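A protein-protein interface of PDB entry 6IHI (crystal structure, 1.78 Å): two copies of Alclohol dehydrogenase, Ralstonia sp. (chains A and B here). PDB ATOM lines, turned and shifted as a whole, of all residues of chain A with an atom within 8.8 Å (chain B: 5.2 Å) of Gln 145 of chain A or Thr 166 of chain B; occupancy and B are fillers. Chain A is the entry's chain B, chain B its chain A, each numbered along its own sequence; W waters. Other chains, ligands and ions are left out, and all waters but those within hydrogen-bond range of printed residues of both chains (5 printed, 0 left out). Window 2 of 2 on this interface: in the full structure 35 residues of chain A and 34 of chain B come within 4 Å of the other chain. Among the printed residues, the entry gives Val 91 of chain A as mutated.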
ATOM      1  N   VAL A  91      25.529  -3.180   3.285  1.00  0.00           N
ATOM      2  CA  VAL A  91      25.473  -2.040   4.192  1.00  0.00           C
ATOM      3  C   VAL A  91      26.510  -2.253   5.281  1.00  0.00           C
ATOM      4  O   VAL A  91      26.543  -3.305   5.933  1.00  0.00           O
ATOM      5  CB  VAL A  91      24.070  -1.835   4.791  1.00  0.00           C
ATOM      6  CG1 VAL A  91      23.557  -3.104   5.450  1.00  0.00           C
ATOM      7  CG2 VAL A  91      24.089  -0.671   5.782  1.00  0.00           C
ATOM      8  N   GLU A  92      27.362  -1.255   5.465  1.00  0.00           N
ATOM      9  CA  GLU A  92      28.324  -1.210   6.552  1.00  0.00           C
ATOM     10  C   GLU A  92      28.176   0.145   7.226  1.00  0.00           C
ATOM     11  O   GLU A  92      28.251   1.178   6.554  1.00  0.00           O
ATOM     12  CB  GLU A  92      29.728  -1.433   5.986  1.00  0.00           C
ATOM     13  CG  GLU A  92      30.896  -1.120   6.860  1.00  0.00           C
ATOM     14  CD  GLU A  92      32.188  -1.485   6.159  1.00  0.00           C
ATOM     15  OE1 GLU A  92      32.129  -2.262   5.179  1.00  0.00           O
ATOM     16  OE2 GLU A  92      33.251  -0.986   6.563  1.00  0.00           O
ATOM     17  N   GLN A  93      27.935   0.145   8.534  1.00  0.00           N
ATOM     18  CA  GLN A  93      27.661   1.381   9.258  1.00  0.00           C
ATOM     19  C   GLN A  93      28.946   2.033   9.760  1.00  0.00           C
ATOM     20  O   GLN A  93      29.739   1.398  10.462  1.00  0.00           O
ATOM     21  CB  GLN A  93      26.721   1.126  10.436  1.00  0.00           C
ATOM     22  CG  GLN A  93      25.411   0.468  10.053  1.00  0.00           C
ATOM     23  CD  GLN A  93      24.362   0.607  11.132  1.00  0.00           C
ATOM     24  OE1 GLN A  93      24.425   1.512  11.962  1.00  0.00           O
ATOM     25  NE2 GLN A  93      23.397  -0.307  11.140  1.00  0.00           N
ATOM     26  N   LYS A  94      29.129   3.306   9.411  1.00  0.00           N
ATOM     27  CA  LYS A  94      30.218   4.131   9.934  1.00  0.00           C
ATOM     28  C   LYS A  94      29.744   5.576   9.985  1.00  0.00           C
ATOM     29  O   LYS A  94      29.168   6.069   9.012  1.00  0.00           O
ATOM     30  CB  LYS A  94      31.481   4.041   9.065  1.00  0.00           C
ATOM     31  CG  LYS A  94      32.170   2.688   9.032  1.00  0.00           C
ATOM     32  CD  LYS A  94      32.798   2.352  10.372  1.00  0.00           C
ATOM     33  CE  LYS A  94      33.614   1.070  10.278  1.00  0.00           C
ATOM     34  NZ  LYS A  94      34.241   0.711  11.580  1.00  0.00           N
ATOM     35  N   THR A  95      29.999   6.254  11.102  1.00  0.00           N
ATOM     36  CA  THR A  95      29.708   7.679  11.169  1.00  0.00           C
ATOM     37  C   THR A  95      30.735   8.467  10.355  1.00  0.00           C
ATOM     38  O   THR A  95      31.796   7.963   9.979  1.00  0.00           O
ATOM     39  CB  THR A  95      29.717   8.172  12.615  1.00  0.00           C
ATOM     40  OG1 THR A  95      31.030   7.998  13.168  1.00  0.00           O
ATOM     41  CG2 THR A  95      28.701   7.405  13.455  1.00  0.00           C
ATOM     42  N   LEU A  96      30.408   9.734  10.094  1.00  0.00           N
ATOM     43  CA  LEU A  96      31.323  10.582   9.336  1.00  0.00           C
ATOM     44  C   LEU A  96      32.711  10.585   9.963  1.00  0.00           C
ATOM     45  O   LEU A  96      33.719  10.446   9.260  1.00  0.00           O
ATOM     46  CB  LEU A  96      30.777  12.005   9.242  1.00  0.00           C
ATOM     47  CG  LEU A  96      31.730  12.999   8.577  1.00  0.00           C
ATOM     48  CD1 LEU A  96      32.145  12.499   7.195  1.00  0.00           C
ATOM     49  CD2 LEU A  96      31.101  14.387   8.497  1.00  0.00           C
ATOM     50  N   GLU A  97      32.777  10.723  11.289  1.00  0.00           N
ATOM     51  CA  GLU A  97      34.064  10.725  11.976  1.00  0.00           C
ATOM     52  C   GLU A  97      34.811   9.415  11.777  1.00  0.00           C
ATOM     53  O   GLU A  97      36.047   9.397  11.804  1.00  0.00           O
ATOM     54  CB  GLU A  97      33.864  10.972  13.470  1.00  0.00           C
ATOM     55  CG  GLU A  97      33.523  12.392  13.857  1.00  0.00           C
ATOM     56  CD  GLU A  97      33.661  12.618  15.348  1.00  0.00           C
ATOM     57  OE1 GLU A  97      33.896  11.628  16.072  1.00  0.00           O
ATOM     58  OE2 GLU A  97      33.543  13.780  15.796  1.00  0.00           O
ATOM     59  N   GLU A  98      34.085   8.312  11.592  1.00  0.00           N
ATOM     60  CA  GLU A  98      34.675   6.983  11.512  1.00  0.00           C
ATOM     61  C   GLU A  98      35.070   6.564  10.101  1.00  0.00           C
ATOM     62  O   GLU A  98      35.797   5.578   9.956  1.00  0.00           O
ATOM     63  CB  GLU A  98      33.703   5.943  12.080  1.00  0.00           C
ATOM     64  CG  GLU A  98      33.472   6.039  13.579  1.00  0.00           C
ATOM     65  CD  GLU A  98      32.306   5.175  14.039  1.00  0.00           C
ATOM     66  OE1 GLU A  98      31.533   4.692  13.176  1.00  0.00           O
ATOM     67  OE2 GLU A  98      32.160   4.982  15.265  1.00  0.00           O
ATOM     68  N   LEU A 142      16.804   9.485   3.244  1.00  0.00           N
ATOM     69  CA  LEU A 142      16.750   9.692   4.688  1.00  0.00           C
ATOM     70  C   LEU A 142      18.112  10.117   5.227  1.00  0.00           C
ATOM     71  O   LEU A 142      19.136  10.048   4.542  1.00  0.00           O
ATOM     72  CB  LEU A 142      16.279   8.422   5.414  1.00  0.00           C
ATOM     73  CG  LEU A 142      14.852   7.950   5.125  1.00  0.00           C
ATOM     74  CD1 LEU A 142      14.573   6.619   5.824  1.00  0.00           C
ATOM     75  CD2 LEU A 142      13.842   9.007   5.543  1.00  0.00           C
ATOM     76  N   GLY A 143      18.108  10.554   6.481  1.00  0.00           N
ATOM     77  CA  GLY A 143      19.334  10.892   7.177  1.00  0.00           C
ATOM     78  C   GLY A 143      19.542   9.963   8.351  1.00  0.00           C
ATOM     79  O   GLY A 143      19.204  10.294   9.493  1.00  0.00           O
ATOM     80  N   LEU A 144      20.078   8.782   8.074  1.00  0.00           N
ATOM     81  CA  LEU A 144      20.198   7.732   9.075  1.00  0.00           C
ATOM     82  C   LEU A 144      21.582   7.769   9.705  1.00  0.00           C
ATOM     83  O   LEU A 144      22.589   7.743   8.994  1.00  0.00           O
ATOM     84  CB  LEU A 144      19.951   6.367   8.437  1.00  0.00           C
ATOM     85  CG  LEU A 144      18.551   6.179   7.850  1.00  0.00           C
ATOM     86  CD1 LEU A 144      18.442   4.857   7.115  1.00  0.00           C
ATOM     87  CD2 LEU A 144      17.519   6.265   8.957  1.00  0.00           C
ATOM     88  N   GLN A 145      21.619   7.831  11.035  1.00  0.00           N
ATOM     89  CA  GLN A 145      22.877   7.786  11.774  1.00  0.00           C
ATOM     90  C   GLN A 145      23.764   6.647  11.283  1.00  0.00           C
ATOM     91  O   GLN A 145      23.318   5.504  11.166  1.00  0.00           O
ATOM     92  CB  GLN A 145      22.577   7.609  13.264  1.00  0.00           C
ATOM     93  CG  GLN A 145      23.796   7.598  14.177  1.00  0.00           C
ATOM     94  CD  GLN A 145      24.402   8.970  14.356  1.00  0.00           C
ATOM     95  OE1 GLN A 145      23.738   9.988  14.146  1.00  0.00           O
ATOM     96  NE2 GLN A 145      25.659   9.009  14.789  1.00  0.00           N
ATOM     97  N   ALA A 146      25.024   6.972  10.983  1.00  0.00           N
ATOM     98  CA  ALA A 146      26.066   6.010  10.630  1.00  0.00           C
ATOM     99  C   ALA A 146      25.807   5.300   9.305  1.00  0.00           C
ATOM    100  O   ALA A 146      26.430   4.273   9.021  1.00  0.00           O
ATOM    101  CB  ALA A 146      26.275   4.975  11.743  1.00  0.00           C
ATOM    102  N   HIS A 147      24.917   5.824   8.466  1.00  0.00           N
ATOM    103  CA  HIS A 147      24.690   5.264   7.140  1.00  0.00           C
ATOM    104  C   HIS A 147      25.259   6.150   6.031  1.00  0.00           C
ATOM    105  O   HIS A 147      24.792   6.087   4.890  1.00  0.00           O
ATOM    106  CB  HIS A 147      23.195   5.027   6.920  1.00  0.00           C
ATOM    107  CG  HIS A 147      22.656   3.845   7.663  1.00  0.00           C
ATOM    108  ND1 HIS A 147      22.478   3.843   9.030  1.00  0.00           N
ATOM    109  CD2 HIS A 147      22.246   2.628   7.227  1.00  0.00           C
ATOM    110  CE1 HIS A 147      21.987   2.674   9.406  1.00  0.00           C
ATOM    111  NE2 HIS A 147      21.835   1.920   8.332  1.00  0.00           N
ATOM    112  N   ASP A 148      26.295   6.943   6.340  1.00  0.00           N
ATOM    113  CA  ASP A 148      26.759   7.989   5.426  1.00  0.00           C
ATOM    114  C   ASP A 148      26.999   7.471   4.014  1.00  0.00           C
ATOM    115  O   ASP A 148      26.389   7.952   3.053  1.00  0.00           O
ATOM    116  CB  ASP A 148      28.052   8.638   5.939  1.00  0.00           C
ATOM    117  CG  ASP A 148      27.940   9.132   7.343  1.00  0.00           C
ATOM    118  OD1 ASP A 148      27.394   8.400   8.187  1.00  0.00           O
ATOM    119  OD2 ASP A 148      28.387  10.275   7.600  1.00  0.00           O
ATOM    120  N   THR A 149      27.911   6.507   3.859  1.00  0.00           N
ATOM    121  CA  THR A 149      28.271   6.085   2.510  1.00  0.00           C
ATOM    122  C   THR A 149      27.176   5.230   1.882  1.00  0.00           C
ATOM    123  O   THR A 149      26.906   5.353   0.682  1.00  0.00           O
ATOM    124  CB  THR A 149      29.610   5.342   2.513  1.00  0.00           C
ATOM    125  OG1 THR A 149      29.504   4.154   3.307  1.00  0.00           O
ATOM    126  CG2 THR A 149      30.721   6.244   3.089  1.00  0.00           C
ATOM    127  N   TYR A 150      26.523   4.375   2.673  1.00  0.00           N
ATOM    128  CA  TYR A 150      25.478   3.510   2.125  1.00  0.00           C
ATOM    129  C   TYR A 150      24.325   4.334   1.573  1.00  0.00           C
ATOM    130  O   TYR A 150      23.863   4.106   0.447  1.00  0.00           O
ATOM    131  CB  TYR A 150      24.968   2.539   3.191  1.00  0.00           C
ATOM    132  CG  TYR A 150      23.852   1.642   2.685  1.00  0.00           C
ATOM    133  CD1 TYR A 150      24.132   0.531   1.900  1.00  0.00           C
ATOM    134  CD2 TYR A 150      22.521   1.919   2.977  1.00  0.00           C
ATOM    135  CE1 TYR A 150      23.114  -0.291   1.424  1.00  0.00           C
ATOM    136  CE2 TYR A 150      21.491   1.096   2.506  1.00  0.00           C
ATOM    137  CZ  TYR A 150      21.801  -0.001   1.729  1.00  0.00           C
ATOM    138  OH  TYR A 150      20.794  -0.818   1.254  1.00  0.00           O
ATOM    139  N   SER A 151      23.840   5.291   2.363  1.00  0.00           N
ATOM    140  CA  SER A 151      22.745   6.142   1.910  1.00  0.00           C
ATOM    141  C   SER A 151      23.134   6.923   0.663  1.00  0.00           C
ATOM    142  O   SER A 151      22.361   7.007  -0.301  1.00  0.00           O
ATOM    143  CB  SER A 151      22.328   7.085   3.033  1.00  0.00           C
ATOM    144  OG  SER A 151      21.834   6.355   4.144  1.00  0.00           O
ATOM    145  N   ARG B 162      21.650  15.177   4.297  1.00  0.00           N
ATOM    146  CA  ARG B 162      20.675  14.583   5.207  1.00  0.00           C
ATOM    147  C   ARG B 162      21.368  13.843   6.344  1.00  0.00           C
ATOM    148  O   ARG B 162      21.053  14.051   7.521  1.00  0.00           O
ATOM    149  CB  ARG B 162      19.763  13.621   4.450  1.00  0.00           C
ATOM    150  CG  ARG B 162      19.022  14.184   3.241  1.00  0.00           C
ATOM    151  CD  ARG B 162      18.086  13.074   2.752  1.00  0.00           C
ATOM    152  NE  ARG B 162      17.440  13.291   1.462  1.00  0.00           N
ATOM    153  CZ  ARG B 162      16.245  13.852   1.302  1.00  0.00           C
ATOM    154  NH1 ARG B 162      15.573  14.310   2.351  1.00  0.00           N
ATOM    155  NH2 ARG B 162      15.724  13.961   0.084  1.00  0.00           N
ATOM    156  N   THR B 163      22.298  12.947   6.002  1.00  0.00           N
ATOM    157  CA  THR B 163      22.972  12.149   7.025  1.00  0.00           C
ATOM    158  C   THR B 163      23.729  13.034   8.007  1.00  0.00           C
ATOM    159  O   THR B 163      23.660  12.830   9.224  1.00  0.00           O
ATOM    160  CB  THR B 163      23.925  11.143   6.371  1.00  0.00           C
ATOM    161  OG1 THR B 163      23.211  10.348   5.413  1.00  0.00           O
ATOM    162  CG2 THR B 163      24.540  10.222   7.429  1.00  0.00           C
ATOM    163  N   TRP B 164      24.452  14.031   7.499  1.00  0.00           N
ATOM    164  CA  TRP B 164      25.256  14.860   8.392  1.00  0.00           C
ATOM    165  C   TRP B 164      24.391  15.796   9.234  1.00  0.00           C
ATOM    166  O   TRP B 164      24.794  16.173  10.336  1.00  0.00           O
ATOM    167  CB  TRP B 164      26.302  15.628   7.581  1.00  0.00           C
ATOM    168  CG  TRP B 164      27.304  14.700   6.941  1.00  0.00           C
ATOM    169  CD1 TRP B 164      27.588  13.417   7.321  1.00  0.00           C
ATOM    170  CD2 TRP B 164      28.128  14.970   5.802  1.00  0.00           C
ATOM    171  NE1 TRP B 164      28.545  12.878   6.499  1.00  0.00           N
ATOM    172  CE2 TRP B 164      28.893  13.811   5.555  1.00  0.00           C
ATOM    173  CE3 TRP B 164      28.295  16.081   4.966  1.00  0.00           C
ATOM    174  CZ2 TRP B 164      29.814  13.734   4.514  1.00  0.00           C
ATOM    175  CZ3 TRP B 164      29.212  16.000   3.930  1.00  0.00           C
ATOM    176  CH2 TRP B 164      29.959  14.838   3.716  1.00  0.00           C
ATOM    177  N   THR B 165      23.209  16.183   8.741  1.00  0.00           N
ATOM    178  CA  THR B 165      22.241  16.873   9.593  1.00  0.00           C
ATOM    179  C   THR B 165      21.946  16.058  10.848  1.00  0.00           C
ATOM    180  O   THR B 165      21.965  16.580  11.968  1.00  0.00           O
ATOM    181  CB  THR B 165      20.946  17.133   8.819  1.00  0.00           C
ATOM    182  OG1 THR B 165      21.169  18.163   7.854  1.00  0.00           O
ATOM    183  CG2 THR B 165      19.831  17.568   9.761  1.00  0.00           C
ATOM    184  N   THR B 166      21.688  14.762  10.671  1.00  0.00           N
ATOM    185  CA  THR B 166      21.396  13.897  11.811  1.00  0.00           C
ATOM    186  C   THR B 166      22.620  13.727  12.705  1.00  0.00           C
ATOM    187  O   THR B 166      22.521  13.832  13.933  1.00  0.00           O
ATOM    188  CB  THR B 166      20.907  12.537  11.309  1.00  0.00           C
ATOM    189  OG1 THR B 166      19.582  12.675  10.786  1.00  0.00           O
ATOM    190  CG2 THR B 166      20.915  11.492  12.430  1.00  0.00           C
ATOM    191  N   GLU B 167      23.788  13.492  12.110  1.00  0.00           N
ATOM    192  CA  GLU B 167      24.955  13.151  12.915  1.00  0.00           C
ATOM    193  C   GLU B 167      25.506  14.353  13.667  1.00  0.00           C
ATOM    194  O   GLU B 167      26.082  14.188  14.751  1.00  0.00           O
ATOM    195  CB  GLU B 167      26.034  12.540  12.028  1.00  0.00           C
ATOM    196  CG  GLU B 167      25.632  11.187  11.481  1.00  0.00           C
ATOM    197  CD  GLU B 167      26.794  10.427  10.908  1.00  0.00           C
ATOM    198  OE1 GLU B 167      27.932  10.947  10.929  1.00  0.00           O
ATOM    199  OE2 GLU B 167      26.563   9.301  10.431  1.00  0.00           O
ATOM    200  N   LEU B 168      25.339  15.557  13.128  1.00  0.00           N
ATOM    201  CA  LEU B 168      25.928  16.750  13.716  1.00  0.00           C
ATOM    202  C   LEU B 168      24.916  17.589  14.479  1.00  0.00           C
ATOM    203  O   LEU B 168      25.250  18.692  14.921  1.00  0.00           O
ATOM    204  CB  LEU B 168      26.604  17.598  12.636  1.00  0.00           C
ATOM    205  CG  LEU B 168      27.650  16.861  11.793  1.00  0.00           C
ATOM    206  CD1 LEU B 168      28.250  17.792  10.741  1.00  0.00           C
ATOM    207  CD2 LEU B 168      28.739  16.272  12.688  1.00  0.00           C
ATOM    208  N   LYS B 169      23.687  17.093  14.647  1.00  0.00           N
ATOM    209  CA  LYS B 169      22.665  17.886  15.320  1.00  0.00           C
ATOM    210  C   LYS B 169      23.031  18.164  16.775  1.00  0.00           C
ATOM    211  O   LYS B 169      22.614  19.186  17.328  1.00  0.00           O
ATOM    212  CB  LYS B 169      21.308  17.186  15.223  1.00  0.00           C
ATOM    213  CG  LYS B 169      21.189  15.896  16.013  1.00  0.00           C
ATOM    214  CD  LYS B 169      19.837  15.245  15.760  1.00  0.00           C
ATOM    215  CE  LYS B 169      19.689  13.951  16.533  1.00  0.00           C
ATOM    216  NZ  LYS B 169      18.421  13.255  16.170  1.00  0.00           N
ATOM    217  N   GLY B 170      23.801  17.272  17.408  1.00  0.00           N
ATOM    218  CA  GLY B 170      24.223  17.505  18.781  1.00  0.00           C
ATOM    219  C   GLY B 170      25.101  18.730  18.932  1.00  0.00           C
ATOM    220  O   GLY B 170      25.147  19.342  20.004  1.00  0.00           O
HETATM  221  O   HOH W   1      26.846  11.599  15.597  1.00  0.00           O
HETATM  222  O   HOH W   2      22.928  11.523  15.806  1.00  0.00           O
HETATM  223  O   HOH W   3      21.031   8.455   5.617  1.00  0.00           O
HETATM  224  O   HOH W   4      30.174  11.767  12.708  1.00  0.00           O
HETATM  225  O   HOH W   5      24.430  10.053   3.216  1.00  0.00           O
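No position is printed for both chains.
Of the 14 pairs that touch across the chains among the printed residues, none has its exchanged pair printed and touching as well.
Printed residues of chain B within 4 Å of Gln 145 of chain A: Thr 166 (3.6 Å) and Glu 167 (3.5 Å).
Of the printed residues of chain A, Thr 166 of chain B touches Gly 143 (2.7 Å) and Gln 145 (3.6 Å).
No residue of chain A comes within 4 Å of Thr 165 of chain B.
Of the printed residues of chain A, Arg 162 of chain B touches Leu 142 and Gly 143.
Printed residues of chain A within 4 Å of Trp 164 of chain B: Leu 96 (3.6 Å) and Asp 148 (2.8 Å).
Of the printed residues of chain B, Thr 95 of chain A touches Glu 167.
Printed residues of chain B within 4 Å of Asp 148 of chain A: Thr 163, Trp 164 and Glu 167.
Of the printed residues of chain B, Leu 142 of chain A touches Arg 162.
The nearest printed residue of chain B that does not touch Gln 145 of chain A is Thr 163 of chain B (5.2 Å).
The nearest printed residue of chain B that does not touch Leu 144 of chain A is Glu 167 of chain B (4.5 Å).
Among the printed residues, pairs that only touch across the chains: Thr 95 of chain A with Glu 167 of chain B, Leu 96 of chain A with Trp 164 of chain B, Leu 142 of chain A with Arg 162 of chain B, Gly 143 of chain A with Arg 162 of chain B, Gly 143 of chain A with Thr 163 of chain B, Leu 144 of chain A with Thr 163 of chain B, Gln 145 of chain A with Thr 166 of chain B, Gln 145 of chain A with Glu 167 of chain B and Asp 148 of chain A with Thr 163 of chain B.
The backbone carbonyl oxygen (O) of Ala 146 of chain A is in hydrogen-bond range of the backbone NH (N) of Lys 94 of chain A, at 2.9 Å.
N of Thr 95 of chain A lies within hydrogen-bond range of OE1 of Glu 98 of chain A, 3.0 Å away.
The backbone NH (N) of Leu 96 of chain A lies within hydrogen-bond range of the side-chain carboxylate (OD2) of Asp 148 of chain A, 3.3 Å away.
The backbone carbonyl oxygen of Gln 145 of chain A is in hydrogen-bond range of a ring nitrogen (ND1) of His 147 of chain A (2.8 Å).
Water W2 bridges the side-chain amide oxygen of Gln 145 of chain A and the backbone carbonyl oxygen of Thr 166 of chain B.
Water W5 bridges OG1 of Thr 163 of chain B (2.5 Å) and O of Asp 148 of chain A (2.9 Å).
Water W3 lies within hydrogen-bond range of N of Leu 144 of chain A (2.7 Å), OG of Ser 151 of chain A (2.7 Å), O of Leu 142 of chain A (2.7 Å) and OG1 of Thr 163 of chain B (2.9 Å).
Water W1 bridges O of Glu 167 of chain B and NE2 of Gln 145 of chain A.
Water W4 lies within hydrogen-bond range of OE1 of Glu 167 of chain B (3.0 Å), N of Glu 97 of chain A (3.1 Å) and N of Leu 96 of chain A (3.3 Å).
Of the 9 printed residues of chain B, 5 touch a printed residue of chain A.
Printed residues of chain B that touch a printed residue of chain A: Arg 162, Thr 163, Trp 164, Thr 166 and Glu 167.
Hydrophobic or aromatic side chains of chain B within 4 Å of the printed part of chain A: Trp 164.
Printed residues of chain A that touch a printed residue of chain B: Thr 95, Leu 96, Leu 142, Gly 143, Leu 144, Gln 145, Ala 146 and Asp 148.
Among the printed residues, 14 pairs touch across the chains.
Among the printed residues, no Asp or Glu carboxylate lies within 4 Å of a Lys or Arg side-chain nitrogen of the other chain.
OD2 of Asp 148 of chain A sits at hydrogen-bond distance from NE1 of Trp 164 of chain B.
OG1 of Thr 166 of chain B sits at hydrogen-bond distance from O of Gly 143 of chain A (2.7 Å).
The backbone NH (N) of Leu 96 of chain A lies within hydrogen-bond range of the side-chain carboxylate (OE1) of Glu 167 of chain B, 2.9 Å away.
The side-chain carboxylate (OE2) of Glu 167 of chain B lies within hydrogen-bond range of the backbone NH (N) of Ala 146 of chain A (2.8 Å).
OE2 of Glu 167 of chain B lies close to OD1 of Asp 148 of chain A (2.6 Å).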
